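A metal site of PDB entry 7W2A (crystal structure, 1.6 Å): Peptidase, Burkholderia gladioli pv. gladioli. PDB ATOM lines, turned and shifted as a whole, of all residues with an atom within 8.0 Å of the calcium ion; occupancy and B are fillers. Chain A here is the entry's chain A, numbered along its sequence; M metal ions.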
ATOM      1  N   PRO A   3      15.321  28.569  -1.490  1.00  0.00           N
ATOM      2  CA  PRO A   3      14.817  27.687  -2.544  1.00  0.00           C
ATOM      3  C   PRO A   3      14.406  28.492  -3.762  1.00  0.00           C
ATOM      4  O   PRO A   3      14.213  29.709  -3.686  1.00  0.00           O
ATOM      5  CB  PRO A   3      13.597  27.040  -1.883  1.00  0.00           C
ATOM      6  CG  PRO A   3      13.038  28.185  -1.042  1.00  0.00           C
ATOM      7  CD  PRO A   3      14.256  28.948  -0.539  1.00  0.00           C
ATOM      8  N   ASN A   4      14.223  27.799  -4.891  1.00  0.00           N
ATOM      9  CA  ASN A   4      13.933  28.459  -6.158  1.00  0.00           C
ATOM     10  C   ASN A   4      12.433  28.545  -6.492  1.00  0.00           C
ATOM     11  O   ASN A   4      12.081  28.876  -7.629  1.00  0.00           O
ATOM     12  CB  ASN A   4      14.682  27.749  -7.299  1.00  0.00           C
ATOM     13  CG  ASN A   4      14.135  26.377  -7.617  1.00  0.00           C
ATOM     14  OD1 ASN A   4      13.159  25.932  -7.021  1.00  0.00           O
ATOM     15  ND2 ASN A   4      14.772  25.676  -8.563  1.00  0.00           N
ATOM     16  N   ASP A   5      11.550  28.266  -5.536  1.00  0.00           N
ATOM     17  CA  ASP A   5      10.133  28.189  -5.874  1.00  0.00           C
ATOM     18  C   ASP A   5       9.587  29.534  -6.334  1.00  0.00           C
ATOM     19  O   ASP A   5       9.926  30.598  -5.790  1.00  0.00           O
ATOM     20  CB  ASP A   5       9.316  27.663  -4.696  1.00  0.00           C
ATOM     21  CG  ASP A   5       9.894  26.377  -4.151  1.00  0.00           C
ATOM     22  OD1 ASP A   5      10.888  26.452  -3.393  1.00  0.00           O
ATOM     23  OD2 ASP A   5       9.375  25.300  -4.499  1.00  0.00           O
ATOM     24  N   THR A   6       8.689  29.465  -7.329  1.00  0.00           N
ATOM     25  CA  THR A   6       8.138  30.644  -7.988  1.00  0.00           C
ATOM     26  C   THR A   6       7.547  31.656  -7.015  1.00  0.00           C
ATOM     27  O   THR A   6       7.714  32.878  -7.196  1.00  0.00           O
ATOM     28  CB  THR A   6       7.074  30.188  -8.972  1.00  0.00           C
ATOM     29  OG1 THR A   6       7.599  29.086  -9.739  1.00  0.00           O
ATOM     30  CG2 THR A   6       6.684  31.339  -9.912  1.00  0.00           C
ATOM     31  N   ARG A   7       6.823  31.186  -6.003  1.00  0.00           N
ATOM     32  CA  ARG A   7       6.082  32.042  -5.097  1.00  0.00           C
ATOM     33  C   ARG A   7       6.769  32.251  -3.754  1.00  0.00           C
ATOM     34  O   ARG A   7       6.198  32.895  -2.872  1.00  0.00           O
ATOM     35  CB  ARG A   7       4.683  31.451  -4.858  1.00  0.00           C
ATOM     36  CG  ARG A   7       3.992  30.963  -6.131  1.00  0.00           C
ATOM     37  CD  ARG A   7       3.562  32.140  -7.013  1.00  0.00           C
ATOM     38  NE  ARG A   7       2.640  33.049  -6.326  1.00  0.00           N
ATOM     39  CZ  ARG A   7       1.329  32.870  -6.245  1.00  0.00           C
ATOM     40  NH1 ARG A   7       0.760  31.797  -6.805  1.00  0.00           N
ATOM     41  NH2 ARG A   7       0.577  33.748  -5.597  1.00  0.00           N
ATOM     42  N   TYR A   8       7.984  31.706  -3.576  1.00  0.00           N
ATOM     43  CA  TYR A   8       8.665  31.828  -2.291  1.00  0.00           C
ATOM     44  C   TYR A   8       8.834  33.291  -1.883  1.00  0.00           C
ATOM     45  O   TYR A   8       8.725  33.633  -0.694  1.00  0.00           O
ATOM     46  CB  TYR A   8      10.011  31.107  -2.349  1.00  0.00           C
ATOM     47  CG  TYR A   8      10.959  31.512  -1.245  1.00  0.00           C
ATOM     48  CD1 TYR A   8      10.787  31.037   0.074  1.00  0.00           C
ATOM     49  CD2 TYR A   8      12.027  32.384  -1.490  1.00  0.00           C
ATOM     50  CE1 TYR A   8      11.621  31.429   1.087  1.00  0.00           C
ATOM     51  CE2 TYR A   8      12.870  32.786  -0.471  1.00  0.00           C
ATOM     52  CZ  TYR A   8      12.676  32.296   0.816  1.00  0.00           C
ATOM     53  OH  TYR A   8      13.519  32.691   1.848  1.00  0.00           O
ATOM     54  N   GLN A  11       6.259  34.653   0.369  1.00  0.00           N
ATOM     55  CA  GLN A  11       6.132  34.014   1.689  1.00  0.00           C
ATOM     56  C   GLN A  11       7.013  34.772   2.685  1.00  0.00           C
ATOM     57  O   GLN A  11       8.077  34.328   3.125  1.00  0.00           O
ATOM     58  CB  GLN A  11       6.500  32.542   1.585  1.00  0.00           C
ATOM     59  CG  GLN A  11       5.577  31.827   0.599  1.00  0.00           C
ATOM     60  CD  GLN A  11       5.808  30.338   0.551  1.00  0.00           C
ATOM     61  OE1 GLN A  11       6.764  29.874  -0.053  1.00  0.00           O
ATOM     62  NE2 GLN A  11       4.916  29.588   1.193  1.00  0.00           N
ATOM     63  N   HIS A  48      -1.899  17.703  -3.485  1.00  0.00           N
ATOM     64  CA  HIS A  48      -1.386  18.793  -4.303  1.00  0.00           C
ATOM     65  C   HIS A  48      -0.027  18.416  -4.886  1.00  0.00           C
ATOM     66  O   HIS A  48       0.816  17.829  -4.202  1.00  0.00           O
ATOM     67  CB  HIS A  48      -1.286  20.021  -3.391  1.00  0.00           C
ATOM     68  CG  HIS A  48      -1.098  21.334  -4.092  1.00  0.00           C
ATOM     69  ND1 HIS A  48      -0.017  21.607  -4.892  1.00  0.00           N
ATOM     70  CD2 HIS A  48      -1.833  22.469  -4.041  1.00  0.00           C
ATOM     71  CE1 HIS A  48      -0.108  22.853  -5.340  1.00  0.00           C
ATOM     72  NE2 HIS A  48      -1.193  23.394  -4.839  1.00  0.00           N
ATOM     73  N   ALA A  49       0.184  18.751  -6.160  1.00  0.00           N
ATOM     74  CA  ALA A  49       1.458  18.421  -6.803  1.00  0.00           C
ATOM     75  C   ALA A  49       2.654  19.020  -6.065  1.00  0.00           C
ATOM     76  O   ALA A  49       3.767  18.477  -6.142  1.00  0.00           O
ATOM     77  CB  ALA A  49       1.451  18.885  -8.261  1.00  0.00           C
ATOM     78  N   ASP A  50       2.447  20.150  -5.372  1.00  0.00           N
ATOM     79  CA  ASP A  50       3.500  20.806  -4.614  1.00  0.00           C
ATOM     80  C   ASP A  50       3.503  20.400  -3.143  1.00  0.00           C
ATOM     81  O   ASP A  50       4.075  21.107  -2.320  1.00  0.00           O
ATOM     82  CB  ASP A  50       3.380  22.326  -4.734  1.00  0.00           C
ATOM     83  CG  ASP A  50       4.736  23.030  -4.764  1.00  0.00           C
ATOM     84  OD1 ASP A  50       5.699  22.438  -5.288  1.00  0.00           O
ATOM     85  OD2 ASP A  50       4.826  24.166  -4.243  1.00  0.00           O
ATOM     86  N   LEU A  51       2.897  19.242  -2.796  1.00  0.00           N
ATOM     87  CA  LEU A  51       2.819  18.796  -1.403  1.00  0.00           C
ATOM     88  C   LEU A  51       2.935  17.277  -1.259  1.00  0.00           C
ATOM     89  O   LEU A  51       3.569  16.786  -0.319  1.00  0.00           O
ATOM     90  CB  LEU A  51       1.499  19.265  -0.790  1.00  0.00           C
ATOM     91  CG  LEU A  51       1.269  18.923   0.685  1.00  0.00           C
ATOM     92  CD1 LEU A  51       2.314  19.614   1.585  1.00  0.00           C
ATOM     93  CD2 LEU A  51      -0.152  19.333   1.077  1.00  0.00           C
ATOM     94  N   ALA A 126       5.538  21.956   2.197  1.00  0.00           N
ATOM     95  CA  ALA A 126       5.379  21.949   0.748  1.00  0.00           C
ATOM     96  C   ALA A 126       6.686  21.516   0.089  1.00  0.00           C
ATOM     97  O   ALA A 126       7.787  21.724   0.625  1.00  0.00           O
ATOM     98  CB  ALA A 126       4.980  23.345   0.233  1.00  0.00           C
ATOM     99  N   VAL A 127       6.552  20.873  -1.084  1.00  0.00           N
ATOM    100  CA  VAL A 127       7.731  20.460  -1.834  1.00  0.00           C
ATOM    101  C   VAL A 127       8.480  21.708  -2.266  1.00  0.00           C
ATOM    102  O   VAL A 127       7.909  22.617  -2.883  1.00  0.00           O
ATOM    103  CB  VAL A 127       7.335  19.574  -3.027  1.00  0.00           C
ATOM    104  CG1 VAL A 127       8.581  19.180  -3.812  1.00  0.00           C
ATOM    105  CG2 VAL A 127       6.614  18.317  -2.528  1.00  0.00           C
ATOM    106  N   SER A 128       9.765  21.766  -1.896  1.00  0.00           N
ATOM    107  CA  SER A 128      10.524  23.001  -1.972  1.00  0.00           C
ATOM    108  C   SER A 128      11.687  22.841  -2.923  1.00  0.00           C
ATOM    109  O   SER A 128      12.184  21.730  -3.138  1.00  0.00           O
ATOM    110  CB  SER A 128      11.025  23.427  -0.587  1.00  0.00           C
ATOM    111  OG  SER A 128       9.911  23.562   0.291  1.00  0.00           O
ATOM    112  N   ASN A 129      12.114  23.972  -3.496  1.00  0.00           N
ATOM    113  CA  ASN A 129      13.221  24.018  -4.452  1.00  0.00           C
ATOM    114  C   ASN A 129      12.924  23.137  -5.670  1.00  0.00           C
ATOM    115  O   ASN A 129      13.847  22.551  -6.255  1.00  0.00           O
ATOM    116  CB  ASN A 129      14.539  23.602  -3.799  1.00  0.00           C
ATOM    117  CG  ASN A 129      15.756  24.202  -4.482  1.00  0.00           C
ATOM    118  OD1 ASN A 129      15.754  25.368  -4.910  1.00  0.00           O
ATOM    119  ND2 ASN A 129      16.823  23.414  -4.578  1.00  0.00           N
ATOM    120  N   ASN A 130      11.644  23.036  -6.045  1.00  0.00           N
ATOM    121  CA  ASN A 130      11.237  22.286  -7.227  1.00  0.00           C
ATOM    122  C   ASN A 130      10.737  23.190  -8.346  1.00  0.00           C
ATOM    123  O   ASN A 130      10.020  22.735  -9.244  1.00  0.00           O
ATOM    124  CB  ASN A 130      10.180  21.230  -6.882  1.00  0.00           C
ATOM    125  CG  ASN A 130       8.854  21.824  -6.460  1.00  0.00           C
ATOM    126  OD1 ASN A 130       8.791  22.973  -6.050  1.00  0.00           O
ATOM    127  ND2 ASN A 130       7.787  21.027  -6.556  1.00  0.00           N
ATOM    128  N   GLY A 131      11.110  24.474  -8.299  1.00  0.00           N
ATOM    129  CA  GLY A 131      10.866  25.348  -9.428  1.00  0.00           C
ATOM    130  C   GLY A 131       9.435  25.738  -9.644  1.00  0.00           C
ATOM    131  O   GLY A 131       9.108  26.249 -10.717  1.00  0.00           O
ATOM    132  N   THR A 132       8.564  25.500  -8.667  1.00  0.00           N
ATOM    133  CA  THR A 132       7.152  25.824  -8.867  1.00  0.00           C
ATOM    134  C   THR A 132       6.480  26.032  -7.525  1.00  0.00           C
ATOM    135  O   THR A 132       6.943  25.518  -6.502  1.00  0.00           O
ATOM    136  CB  THR A 132       6.458  24.726  -9.689  1.00  0.00           C
ATOM    137  OG1 THR A 132       5.205  25.210 -10.173  1.00  0.00           O
ATOM    138  CG2 THR A 132       6.221  23.481  -8.855  1.00  0.00           C
ATOM    139  N   GLY A 133       5.405  26.801  -7.533  1.00  0.00           N
ATOM    140  CA  GLY A 133       4.585  26.924  -6.341  1.00  0.00           C
ATOM    141  C   GLY A 133       5.308  27.575  -5.183  1.00  0.00           C
ATOM    142  O   GLY A 133       6.070  28.539  -5.351  1.00  0.00           O
ATOM    143  N   VAL A 134       5.080  27.039  -3.983  1.00  0.00           N
ATOM    144  CA  VAL A 134       5.565  27.623  -2.736  1.00  0.00           C
ATOM    145  C   VAL A 134       6.680  26.769  -2.146  1.00  0.00           C
ATOM    146  O   VAL A 134       7.008  25.698  -2.671  1.00  0.00           O
ATOM    147  CB  VAL A 134       4.417  27.772  -1.711  1.00  0.00           C
ATOM    148  CG1 VAL A 134       3.457  28.870  -2.176  1.00  0.00           C
ATOM    149  CG2 VAL A 134       3.669  26.432  -1.552  1.00  0.00           C
ATOM    150  N   ALA A 135       7.268  27.223  -1.042  1.00  0.00           N
ATOM    151  CA  ALA A 135       8.175  26.416  -0.243  1.00  0.00           C
ATOM    152  C   ALA A 135       7.526  26.083   1.099  1.00  0.00           C
ATOM    153  O   ALA A 135       6.554  26.706   1.520  1.00  0.00           O
ATOM    154  CB  ALA A 135       9.520  27.121  -0.021  1.00  0.00           C
ATOM    155  N   GLY A 136       8.093  25.076   1.771  1.00  0.00           N
ATOM    156  CA  GLY A 136       7.751  24.750   3.138  1.00  0.00           C
ATOM    157  C   GLY A 136       8.952  24.937   4.046  1.00  0.00           C
ATOM    158  O   GLY A 136      10.082  25.148   3.595  1.00  0.00           O
ATOM    159  N   THR A 268      -0.232  26.158  -0.057  1.00  0.00           N
ATOM    160  CA  THR A 268      -0.969  25.255  -0.943  1.00  0.00           C
ATOM    161  C   THR A 268      -2.468  25.233  -0.606  1.00  0.00           C
ATOM    162  O   THR A 268      -2.849  25.250   0.563  1.00  0.00           O
ATOM    163  CB  THR A 268      -0.395  23.845  -0.819  1.00  0.00           C
ATOM    164  OG1 THR A 268      -0.089  23.593   0.558  1.00  0.00           O
ATOM    165  CG2 THR A 268       0.899  23.718  -1.591  1.00  0.00           C
ATOM    166  N   TYR A 281      -2.942  27.974  -4.979  1.00  0.00           N
ATOM    167  CA  TYR A 281      -2.237  28.580  -3.860  1.00  0.00           C
ATOM    168  C   TYR A 281      -3.112  29.715  -3.353  1.00  0.00           C
ATOM    169  O   TYR A 281      -3.806  30.360  -4.150  1.00  0.00           O
ATOM    170  CB  TYR A 281      -0.836  29.104  -4.266  1.00  0.00           C
ATOM    171  CG  TYR A 281      -0.013  28.015  -4.926  1.00  0.00           C
ATOM    172  CD1 TYR A 281       0.643  27.059  -4.171  1.00  0.00           C
ATOM    173  CD2 TYR A 281       0.041  27.910  -6.318  1.00  0.00           C
ATOM    174  CE1 TYR A 281       1.363  26.032  -4.775  1.00  0.00           C
ATOM    175  CE2 TYR A 281       0.762  26.889  -6.935  1.00  0.00           C
ATOM    176  CZ  TYR A 281       1.423  25.944  -6.150  1.00  0.00           C
ATOM    177  OH  TYR A 281       2.115  24.933  -6.756  1.00  0.00           O
HETATM  178 CA    CA M   1       7.320  24.182  -4.544  1.00  0.00          CA
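Gly 133 touches the calcium ion (C to CA, 3.996 Å).
Of the 24 residues printed, 7 come within 4 Å of the calcium ion.
The nearest printed residue that does not touch the calcium ion is Ser 128 (4.3 Å).
The side-chain carboxylate (OD1) of Asp 5 is in hydrogen-bond range of the backbone NH (N) of Asn 129 (2.8 Å).
The side-chain amide oxygen (OD1) of Asn 4 is in hydrogen-bond range of the backbone NH (N) of Asn 130.
N of Asp 50 lies within hydrogen-bond range of ND1 of His 48 (2.9 Å).
The backbone carbonyl oxygen of Gly 133 lies within hydrogen-bond range of the backbone NH of Thr 6, 3.4 Å away.
N of Arg 7 sits at hydrogen-bond distance from O of Gly 133, 2.8 Å away.
The calcium ion is bound by the side-chain carboxylate (OD2) of Asp 5, the backbone carbonyl oxygen (O) of Val 127, the backbone carbonyl oxygen (O) of Thr 132, the side-chain amide oxygen (OD1) of Asn 130, the backbone carbonyl oxygen (O) of Val 134, the side-chain carboxylate (OD1) of Asp 50 and the side-chain carboxylate (OD2) of Asp 50.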
